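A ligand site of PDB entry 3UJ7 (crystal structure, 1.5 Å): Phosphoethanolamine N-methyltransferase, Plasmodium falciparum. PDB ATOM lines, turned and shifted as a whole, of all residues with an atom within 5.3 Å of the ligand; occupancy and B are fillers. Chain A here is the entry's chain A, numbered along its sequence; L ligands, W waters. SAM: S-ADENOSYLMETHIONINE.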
ATOM      1  N   LEU A  14      29.652 -28.897   0.875  1.00  0.00           N
ATOM      2  CA  LEU A  14      28.777 -27.752   0.675  1.00  0.00           C
ATOM      3  C   LEU A  14      28.713 -27.322  -0.799  1.00  0.00           C
ATOM      4  O   LEU A  14      27.634 -27.047  -1.329  1.00  0.00           O
ATOM      5  CB  LEU A  14      29.218 -26.602   1.575  1.00  0.00           C
ATOM      6  CG  LEU A  14      29.071 -26.824   3.087  1.00  0.00           C
ATOM      7  CD1 LEU A  14      29.820 -25.760   3.883  1.00  0.00           C
ATOM      8  CD2 LEU A  14      27.604 -26.849   3.477  1.00  0.00           C
ATOM      9  N   TYR A  19      25.087 -25.911  -1.851  1.00  0.00           N
ATOM     10  CA  TYR A  19      25.485 -24.649  -2.452  1.00  0.00           C
ATOM     11  C   TYR A  19      26.162 -24.805  -3.807  1.00  0.00           C
ATOM     12  O   TYR A  19      27.163 -24.153  -4.099  1.00  0.00           O
ATOM     13  CB  TYR A  19      26.349 -23.830  -1.472  1.00  0.00           C
ATOM     14  CG  TYR A  19      25.657 -23.525  -0.166  1.00  0.00           C
ATOM     15  CD1 TYR A  19      24.512 -22.737  -0.125  1.00  0.00           C
ATOM     16  CD2 TYR A  19      26.158 -24.007   1.027  1.00  0.00           C
ATOM     17  CE1 TYR A  19      23.880 -22.440   1.097  1.00  0.00           C
ATOM     18  CE2 TYR A  19      25.545 -23.721   2.241  1.00  0.00           C
ATOM     19  CZ  TYR A  19      24.412 -22.942   2.271  1.00  0.00           C
ATOM     20  OH  TYR A  19      23.822 -22.678   3.496  1.00  0.00           O
ATOM     21  N   ASN A  34      21.000 -10.943  -4.158  1.00  0.00           N
ATOM     22  CA  ASN A  34      22.204 -10.847  -3.325  1.00  0.00           C
ATOM     23  C   ASN A  34      22.096 -11.524  -1.963  1.00  0.00           C
ATOM     24  O   ASN A  34      23.020 -11.445  -1.158  1.00  0.00           O
ATOM     25  CB  ASN A  34      22.637  -9.392  -3.125  1.00  0.00           C
ATOM     26  CG  ASN A  34      22.914  -8.679  -4.423  1.00  0.00           C
ATOM     27  OD1 ASN A  34      23.462  -9.261  -5.357  1.00  0.00           O
ATOM     28  ND2 ASN A  34      22.498  -7.428  -4.506  1.00  0.00           N
ATOM     29  N   TYR A  35      20.993 -12.224  -1.715  1.00  0.00           N
ATOM     30  CA  TYR A  35      20.792 -12.887  -0.438  1.00  0.00           C
ATOM     31  C   TYR A  35      20.531 -14.368  -0.587  1.00  0.00           C
ATOM     32  O   TYR A  35      19.846 -14.799  -1.520  1.00  0.00           O
ATOM     33  CB  TYR A  35      19.627 -12.238   0.322  1.00  0.00           C
ATOM     34  CG  TYR A  35      19.967 -10.871   0.850  1.00  0.00           C
ATOM     35  CD1 TYR A  35      19.717  -9.726   0.096  1.00  0.00           C
ATOM     36  CD2 TYR A  35      20.584 -10.726   2.090  1.00  0.00           C
ATOM     37  CE1 TYR A  35      20.039  -8.486   0.568  1.00  0.00           C
ATOM     38  CE2 TYR A  35      20.914  -9.484   2.578  1.00  0.00           C
ATOM     39  CZ  TYR A  35      20.637  -8.363   1.815  1.00  0.00           C
ATOM     40  OH  TYR A  35      20.962  -7.134   2.307  1.00  0.00           O
ATOM     41  N   ILE A  36      21.060 -15.159   0.338  1.00  0.00           N
ATOM     42  CA  ILE A  36      20.674 -16.555   0.427  1.00  0.00           C
ATOM     43  C   ILE A  36      20.289 -16.937   1.860  1.00  0.00           C
ATOM     44  O   ILE A  36      20.503 -18.061   2.293  1.00  0.00           O
ATOM     45  CB  ILE A  36      21.756 -17.520  -0.146  1.00  0.00           C
ATOM     46  CG1 ILE A  36      23.117 -17.250   0.483  1.00  0.00           C
ATOM     47  CG2 ILE A  36      21.827 -17.376  -1.672  1.00  0.00           C
ATOM     48  CD1 ILE A  36      24.262 -18.086  -0.131  1.00  0.00           C
ATOM     49  N   SER A  37      19.699 -16.003   2.587  1.00  0.00           N
ATOM     50  CA  SER A  37      19.142 -16.318   3.882  1.00  0.00           C
ATOM     51  C   SER A  37      17.920 -15.505   4.244  1.00  0.00           C
ATOM     52  O   SER A  37      17.599 -14.572   3.642  1.00  0.00           O
ATOM     53  CB  SER A  37      20.192 -16.201   4.984  1.00  0.00           C
ATOM     54  OG  SER A  37      20.354 -14.874   5.342  1.00  0.00           O
ATOM     55  N   ASP A  61      32.013 -10.228   8.175  1.00  0.00           N
ATOM     56  CA  ASP A  61      30.787 -10.998   7.932  1.00  0.00           C
ATOM     57  C   ASP A  61      31.203 -12.468   7.761  1.00  0.00           C
ATOM     58  O   ASP A  61      31.872 -12.841   6.782  1.00  0.00           O
ATOM     59  CB  ASP A  61      30.032 -10.472   6.688  1.00  0.00           C
ATOM     60  CG  ASP A  61      28.682 -11.173   6.473  1.00  0.00           C
ATOM     61  OD1 ASP A  61      28.383 -12.182   7.139  1.00  0.00           O
ATOM     62  OD2 ASP A  61      27.905 -10.713   5.602  1.00  0.00           O
ATOM     63  N   ILE A  62      30.817 -13.295   8.727  1.00  0.00           N
ATOM     64  CA  ILE A  62      31.131 -14.709   8.699  1.00  0.00           C
ATOM     65  C   ILE A  62      30.051 -15.498   7.947  1.00  0.00           C
ATOM     66  O   ILE A  62      28.894 -15.558   8.390  1.00  0.00           O
ATOM     67  CB  ILE A  62      31.235 -15.242  10.136  1.00  0.00           C
ATOM     68  CG1 ILE A  62      32.397 -14.555  10.855  1.00  0.00           C
ATOM     69  CG2 ILE A  62      31.435 -16.763  10.127  1.00  0.00           C
ATOM     70  CD1 ILE A  62      32.448 -14.886  12.340  1.00  0.00           C
ATOM     71  N   GLY A  63      30.437 -16.089   6.816  1.00  0.00           N
ATOM     72  CA  GLY A  63      29.513 -16.741   5.914  1.00  0.00           C
ATOM     73  C   GLY A  63      28.797 -15.722   5.044  1.00  0.00           C
ATOM     74  O   GLY A  63      27.580 -15.661   5.037  1.00  0.00           O
ATOM     75  N   SER A  64      29.562 -14.910   4.322  1.00  0.00           N
ATOM     76  CA  SER A  64      29.045 -13.741   3.639  1.00  0.00           C
ATOM     77  C   SER A  64      28.166 -13.997   2.397  1.00  0.00           C
ATOM     78  O   SER A  64      27.503 -13.076   1.905  1.00  0.00           O
ATOM     79  CB  SER A  64      30.209 -12.800   3.280  1.00  0.00           C
ATOM     80  OG  SER A  64      31.278 -13.526   2.682  1.00  0.00           O
ATOM     81  N   GLY A  65      28.170 -15.222   1.889  1.00  0.00           N
ATOM     82  CA  GLY A  65      27.285 -15.591   0.794  1.00  0.00           C
ATOM     83  C   GLY A  65      27.490 -14.783  -0.482  1.00  0.00           C
ATOM     84  O   GLY A  65      28.613 -14.614  -0.951  1.00  0.00           O
ATOM     85  N   LEU A  66      26.384 -14.283  -1.048  1.00  0.00           N
ATOM     86  CA  LEU A  66      26.439 -13.462  -2.260  1.00  0.00           C
ATOM     87  C   LEU A  66      26.745 -12.001  -1.967  1.00  0.00           C
ATOM     88  O   LEU A  66      26.818 -11.168  -2.874  1.00  0.00           O
ATOM     89  CB  LEU A  66      25.130 -13.541  -3.033  1.00  0.00           C
ATOM     90  CG  LEU A  66      24.803 -14.895  -3.643  1.00  0.00           C
ATOM     91  CD1 LEU A  66      23.375 -14.890  -4.155  1.00  0.00           C
ATOM     92  CD2 LEU A  66      25.781 -15.214  -4.760  1.00  0.00           C
ATOM     93  N   ILE A  84      33.813 -13.512   4.698  1.00  0.00           N
ATOM     94  CA  ILE A  84      34.505 -14.780   4.546  1.00  0.00           C
ATOM     95  C   ILE A  84      33.453 -15.840   4.265  1.00  0.00           C
ATOM     96  O   ILE A  84      32.453 -15.949   4.983  1.00  0.00           O
ATOM     97  CB  ILE A  84      35.249 -15.170   5.839  1.00  0.00           C
ATOM     98  CG1 ILE A  84      36.355 -14.151   6.157  1.00  0.00           C
ATOM     99  CG2 ILE A  84      35.840 -16.579   5.697  1.00  0.00           C
ATOM    100  CD1 ILE A  84      37.576 -14.261   5.253  1.00  0.00           C
ATOM    101  N   ASP A  85      33.670 -16.626   3.223  1.00  0.00           N
ATOM    102  CA  ASP A  85      32.787 -17.732   2.940  1.00  0.00           C
ATOM    103  C   ASP A  85      33.610 -18.912   2.440  1.00  0.00           C
ATOM    104  O   ASP A  85      34.556 -18.725   1.698  1.00  0.00           O
ATOM    105  CB  ASP A  85      31.747 -17.314   1.891  1.00  0.00           C
ATOM    106  CG  ASP A  85      30.540 -18.221   1.885  1.00  0.00           C
ATOM    107  OD1 ASP A  85      30.688 -19.384   1.442  1.00  0.00           O
ATOM    108  OD2 ASP A  85      29.461 -17.797   2.339  1.00  0.00           O
ATOM    109  N   ILE A  86      33.262 -20.114   2.866  1.00  0.00           N
ATOM    110  CA  ILE A  86      34.059 -21.293   2.571  1.00  0.00           C
ATOM    111  C   ILE A  86      33.866 -21.772   1.128  1.00  0.00           C
ATOM    112  O   ILE A  86      34.726 -22.456   0.561  1.00  0.00           O
ATOM    113  CB  ILE A  86      33.765 -22.432   3.585  1.00  0.00           C
ATOM    114  CG1 ILE A  86      34.841 -23.518   3.517  1.00  0.00           C
ATOM    115  CG2 ILE A  86      32.360 -22.987   3.395  1.00  0.00           C
ATOM    116  CD1 ILE A  86      34.650 -24.615   4.562  1.00  0.00           C
ATOM    117  N   CYS A  87      32.721 -21.410   0.539  1.00  0.00           N
ATOM    118  CA  CYS A  87      32.397 -21.867  -0.818  1.00  0.00           C
ATOM    119  C   CYS A  87      32.976 -20.960  -1.899  1.00  0.00           C
ATOM    120  O   CYS A  87      32.535 -19.826  -2.081  1.00  0.00           O
ATOM    121  CB  CYS A  87      30.895 -21.980  -0.996  1.00  0.00           C
ATOM    122  SG  CYS A  87      30.177 -23.373  -0.086  1.00  0.00           S
ATOM    123  N   ILE A  90      30.555 -19.445  -4.502  1.00  0.00           N
ATOM    124  CA  ILE A  90      29.725 -18.367  -3.975  1.00  0.00           C
ATOM    125  C   ILE A  90      30.514 -17.060  -3.886  1.00  0.00           C
ATOM    126  O   ILE A  90      30.033 -15.992  -4.222  1.00  0.00           O
ATOM    127  CB  ILE A  90      29.153 -18.745  -2.608  1.00  0.00           C
ATOM    128  CG1 ILE A  90      28.141 -19.885  -2.759  1.00  0.00           C
ATOM    129  CG2 ILE A  90      28.539 -17.522  -1.936  1.00  0.00           C
ATOM    130  CD1 ILE A  90      27.515 -20.304  -1.449  1.00  0.00           C
ATOM    131  N   ASN A 109      37.479 -18.815   2.286  1.00  0.00           N
ATOM    132  CA  ASN A 109      38.271 -19.429   3.340  1.00  0.00           C
ATOM    133  C   ASN A 109      37.341 -20.066   4.364  1.00  0.00           C
ATOM    134  O   ASN A 109      36.182 -19.662   4.489  1.00  0.00           O
ATOM    135  CB  ASN A 109      39.144 -18.376   4.007  1.00  0.00           C
ATOM    136  CG  ASN A 109      40.510 -18.896   4.399  1.00  0.00           C
ATOM    137  OD1 ASN A 109      40.635 -19.859   5.156  1.00  0.00           O
ATOM    138  ND2 ASN A 109      41.548 -18.252   3.890  1.00  0.00           N
ATOM    139  N   ASP A 110      37.829 -21.065   5.081  1.00  0.00           N
ATOM    140  CA  ASP A 110      37.119 -21.635   6.222  1.00  0.00           C
ATOM    141  C   ASP A 110      37.353 -20.692   7.396  1.00  0.00           C
ATOM    142  O   ASP A 110      38.498 -20.452   7.754  1.00  0.00           O
ATOM    143  CB  ASP A 110      37.703 -23.011   6.520  1.00  0.00           C
ATOM    144  CG  ASP A 110      36.984 -23.758   7.635  1.00  0.00           C
ATOM    145  OD1 ASP A 110      36.208 -23.138   8.400  1.00  0.00           O
ATOM    146  OD2 ASP A 110      37.208 -24.982   7.750  1.00  0.00           O
ATOM    147  N   ILE A 111      36.295 -20.149   7.972  1.00  0.00           N
ATOM    148  CA  ILE A 111      36.439 -19.267   9.125  1.00  0.00           C
ATOM    149  C   ILE A 111      37.220 -19.913  10.275  1.00  0.00           C
ATOM    150  O   ILE A 111      37.893 -19.229  11.055  1.00  0.00           O
ATOM    151  CB  ILE A 111      35.078 -18.721   9.616  1.00  0.00           C
ATOM    152  CG1 ILE A 111      35.309 -17.511  10.530  1.00  0.00           C
ATOM    153  CG2 ILE A 111      34.264 -19.810  10.303  1.00  0.00           C
ATOM    154  CD1 ILE A 111      36.008 -16.356   9.827  1.00  0.00           C
ATOM    155  N   LEU A 112      37.146 -21.228  10.383  1.00  0.00           N
ATOM    156  CA  LEU A 112      37.814 -21.928  11.484  1.00  0.00           C
ATOM    157  C   LEU A 112      39.333 -21.908  11.371  1.00  0.00           C
ATOM    158  O   LEU A 112      40.033 -22.117  12.368  1.00  0.00           O
ATOM    159  CB  LEU A 112      37.337 -23.379  11.564  1.00  0.00           C
ATOM    160  CG  LEU A 112      35.866 -23.549  11.953  1.00  0.00           C
ATOM    161  CD1 LEU A 112      35.480 -25.016  11.855  1.00  0.00           C
ATOM    162  CD2 LEU A 112      35.592 -23.017  13.350  1.00  0.00           C
ATOM    163  N   ARG A 127      24.924 -14.242   9.587  1.00  0.00           N
ATOM    164  CA  ARG A 127      23.516 -14.506   9.351  1.00  0.00           C
ATOM    165  C   ARG A 127      23.315 -15.913   8.823  1.00  0.00           C
ATOM    166  O   ARG A 127      23.639 -16.192   7.655  1.00  0.00           O
ATOM    167  CB  ARG A 127      22.948 -13.492   8.351  1.00  0.00           C
ATOM    168  CG  ARG A 127      23.083 -12.060   8.786  1.00  0.00           C
ATOM    169  CD  ARG A 127      22.149 -11.731   9.958  1.00  0.00           C
ATOM    170  NE  ARG A 127      20.772 -12.069   9.625  1.00  0.00           N
ATOM    171  CZ  ARG A 127      19.999 -11.355   8.809  1.00  0.00           C
ATOM    172  NH1 ARG A 127      20.459 -10.225   8.270  1.00  0.00           N
ATOM    173  NH2 ARG A 127      18.766 -11.751   8.562  1.00  0.00           N
ATOM    174  N   ASP A 128      22.790 -16.782   9.677  1.00  0.00           N
ATOM    175  CA  ASP A 128      22.405 -18.144   9.304  1.00  0.00           C
ATOM    176  C   ASP A 128      23.516 -18.938   8.616  1.00  0.00           C
ATOM    177  O   ASP A 128      23.319 -19.570   7.576  1.00  0.00           O
ATOM    178  CB  ASP A 128      21.132 -18.138   8.452  1.00  0.00           C
ATOM    179  CG  ASP A 128      19.977 -17.401   9.114  1.00  0.00           C
ATOM    180  OD1 ASP A 128      20.055 -17.074  10.332  1.00  0.00           O
ATOM    181  OD2 ASP A 128      18.974 -17.151   8.409  1.00  0.00           O
ATOM    182  N   ALA A 129      24.689 -18.926   9.235  1.00  0.00           N
ATOM    183  CA  ALA A 129      25.837 -19.615   8.714  1.00  0.00           C
ATOM    184  C   ALA A 129      26.432 -20.613   9.717  1.00  0.00           C
ATOM    185  O   ALA A 129      26.966 -21.638   9.331  1.00  0.00           O
ATOM    186  CB  ALA A 129      26.897 -18.591   8.270  1.00  0.00           C
ATOM    187  N   HIS A 132      26.142 -24.607  10.224  1.00  0.00           N
ATOM    188  CA  HIS A 132      26.977 -25.588   9.534  1.00  0.00           C
ATOM    189  C   HIS A 132      28.087 -26.180  10.416  1.00  0.00           C
ATOM    190  O   HIS A 132      28.652 -27.237  10.085  1.00  0.00           O
ATOM    191  CB  HIS A 132      27.586 -24.960   8.265  1.00  0.00           C
ATOM    192  CG  HIS A 132      26.594 -24.676   7.193  1.00  0.00           C
ATOM    193  ND1 HIS A 132      25.961 -25.682   6.484  1.00  0.00           N
ATOM    194  CD2 HIS A 132      26.108 -23.516   6.687  1.00  0.00           C
ATOM    195  CE1 HIS A 132      25.141 -25.157   5.611  1.00  0.00           C
ATOM    196  NE2 HIS A 132      25.209 -23.844   5.704  1.00  0.00           N
ATOM    197  N   LEU A 133      28.380 -25.526  11.534  1.00  0.00           N
ATOM    198  CA  LEU A 133      29.508 -25.923  12.374  1.00  0.00           C
ATOM    199  C   LEU A 133      29.074 -26.910  13.464  1.00  0.00           C
ATOM    200  O   LEU A 133      27.993 -26.789  14.016  1.00  0.00           O
ATOM    201  CB  LEU A 133      30.142 -24.687  13.025  1.00  0.00           C
ATOM    202  CG  LEU A 133      31.126 -23.841  12.203  1.00  0.00           C
ATOM    203  CD1 LEU A 133      30.551 -23.423  10.868  1.00  0.00           C
ATOM    204  CD2 LEU A 133      31.562 -22.617  12.993  1.00  0.00           C
HETATM  205  N   SAM L   1      25.040 -14.432   5.255  1.00  0.00           N
HETATM  206  CA  SAM L   1      24.538 -15.039   4.036  1.00  0.00           C
HETATM  207  C   SAM L   1      23.208 -14.417   3.674  1.00  0.00           C
HETATM  208  O   SAM L   1      22.533 -13.898   4.560  1.00  0.00           O
HETATM  209  OXT SAM L   1      22.764 -14.428   2.525  1.00  0.00           O
HETATM  210  CB  SAM L   1      24.240 -16.501   4.346  1.00  0.00           C
HETATM  211  CG  SAM L   1      24.892 -17.517   3.428  1.00  0.00           C
HETATM  212  SD  SAM L   1      24.136 -19.129   3.741  1.00  0.00           S
HETATM  213  CE  SAM L   1      22.813 -18.705   4.912  1.00  0.00           C
HETATM  214  C5' SAM L   1      25.380 -19.917   4.789  1.00  0.00           C
HETATM  215  C4' SAM L   1      26.812 -19.623   4.321  1.00  0.00           C
HETATM  216  O4' SAM L   1      27.733 -20.061   5.297  1.00  0.00           O
HETATM  217  C3' SAM L   1      27.153 -20.368   3.035  1.00  0.00           C
HETATM  218  O3' SAM L   1      27.397 -19.440   1.989  1.00  0.00           O
HETATM  219  C2' SAM L   1      28.389 -21.195   3.374  1.00  0.00           C
HETATM  220  O2' SAM L   1      29.356 -21.215   2.345  1.00  0.00           O
HETATM  221  C1' SAM L   1      28.910 -20.499   4.635  1.00  0.00           C
HETATM  222  N9  SAM L   1      29.782 -21.358   5.475  1.00  0.00           N
HETATM  223  C8  SAM L   1      29.509 -22.601   5.981  1.00  0.00           C
HETATM  224  N7  SAM L   1      30.568 -23.030   6.705  1.00  0.00           N
HETATM  225  C5  SAM L   1      31.533 -22.072   6.666  1.00  0.00           C
HETATM  226  C6  SAM L   1      32.796 -21.994   7.219  1.00  0.00           C
HETATM  227  N6  SAM L   1      33.303 -22.999   7.939  1.00  0.00           N
HETATM  228  N1  SAM L   1      33.557 -20.870   6.990  1.00  0.00           N
HETATM  229  C2  SAM L   1      33.044 -19.831   6.247  1.00  0.00           C
HETATM  230  N3  SAM L   1      31.794 -19.909   5.687  1.00  0.00           N
HETATM  231  C4  SAM L   1      31.041 -21.017   5.902  1.00  0.00           C
HETATM  232  O   HOH W   1      24.680 -11.497   2.757  1.00  0.00           O
HETATM  233  O   HOH W   2      21.068 -11.786   5.451  1.00  0.00           O
HETATM  234  O   HOH W   3      25.410 -11.757   5.250  1.00  0.00           O
HETATM  235  O   HOH W   4      26.711 -13.961   7.409  1.00  0.00           O
HETATM  236  O   HOH W   5      24.137 -13.356   0.675  1.00  0.00           O
HETATM  237  O   HOH W   6      31.419 -25.602   7.519  1.00  0.00           O
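An oxygen (O2') of the ligand lies within hydrogen-bond range of the side-chain carboxylate of Asp 85. N of Ser 37 lies within hydrogen-bond range of OXT of the ligand (3.4 Å). An oxygen (O) of the ligand lies within hydrogen-bond range of the side-chain hydroxyl (OG) of Ser 37. The backbone carbonyl oxygen (O) of Gly 63 is in hydrogen-bond range of a nitrogen (N) of the ligand, 2.8 Å away. N of Ile 36 is in hydrogen-bond range of OXT of the ligand (2.9 Å). A nitrogen (N6) of the ligand is in hydrogen-bond range of the side-chain carboxylate of Asp 110 (2.9 Å). N of Ile 111 is in hydrogen-bond range of N1 of the ligand, at 3.0 Å. N3 of the ligand is in hydrogen-bond range of N of Ile 86. The backbone carbonyl oxygen (O) of Arg 127 sits at hydrogen-bond distance from a nitrogen (N) of the ligand (3.3 Å). The side-chain sulfur (SG) of Cys 87 sits at hydrogen-bond distance from an oxygen (O2') of the ligand, 3.4 Å away.
OD1 of Asp 85 sits at hydrogen-bond distance from N of Cys 87 (3.0 Å). O of Asp 85 is in hydrogen-bond range of N of Asn 109. N of Gly 65 sits at hydrogen-bond distance from OD2 of Asp 85 (2.9 Å). The backbone carbonyl oxygen (O) of Ile 84 lies within hydrogen-bond range of the backbone NH (N) of Gly 63, 2.7 Å away. The backbone NH (N) of Leu 112 sits at hydrogen-bond distance from the side-chain carboxylate (OD1) of Asp 110, at 2.9 Å. The backbone carbonyl oxygen of Asn 109 lies close to the backbone NH of Ile 86 (3.4 Å). The side-chain hydroxyl (OH) of Tyr 19 sits at hydrogen-bond distance from a ring nitrogen (NE2) of His 132, 2.9 Å away. The backbone NH (N) of Tyr 19 lies within hydrogen-bond range of the backbone carbonyl oxygen (O) of Leu 14.
Water W5 lies within hydrogen-bond range of an oxygen (OXT) of the ligand (2.5 Å), the backbone carbonyl oxygen of Asn 34 (2.9 Å) and the backbone NH of Leu 66 (3.0 Å). Water W3 lies within hydrogen-bond range of N of the ligand (2.7 Å) and OD2 of Asp 61 (2.7 Å). Water W2 lies within hydrogen-bond range of an oxygen (O) of the ligand (2.7 Å), the side-chain hydroxyl (OG) of Ser 37 (3.2 Å) and the guanidinium group (NH1) of Arg 127 (3.3 Å).
A sulfur (SD) of the ligand sits close to the side-chain hydroxyl (OH) of Tyr 19 (3.6 Å). Merely in contact with the ligand: Asp 128, Ala 129, Ile 90, His 132, Asn 109, Leu 14 and Tyr 35. Hydrophobic or aromatic side chains that line the ligand: Leu 14, Tyr 19, Ile 36, Ile 86, Ile 90, Ile 111, Ala 129 and His 132. Within 4 Å of the ligand: Leu 14, Tyr 19, Tyr 35, Ile 36, Ser 37, Gly 63, Asp 85, Ile 86, Cys 87, Ile 90, Asn 109, Asp 110, Ile 111, Arg 127, Asp 128, Ala 129 and His 132.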
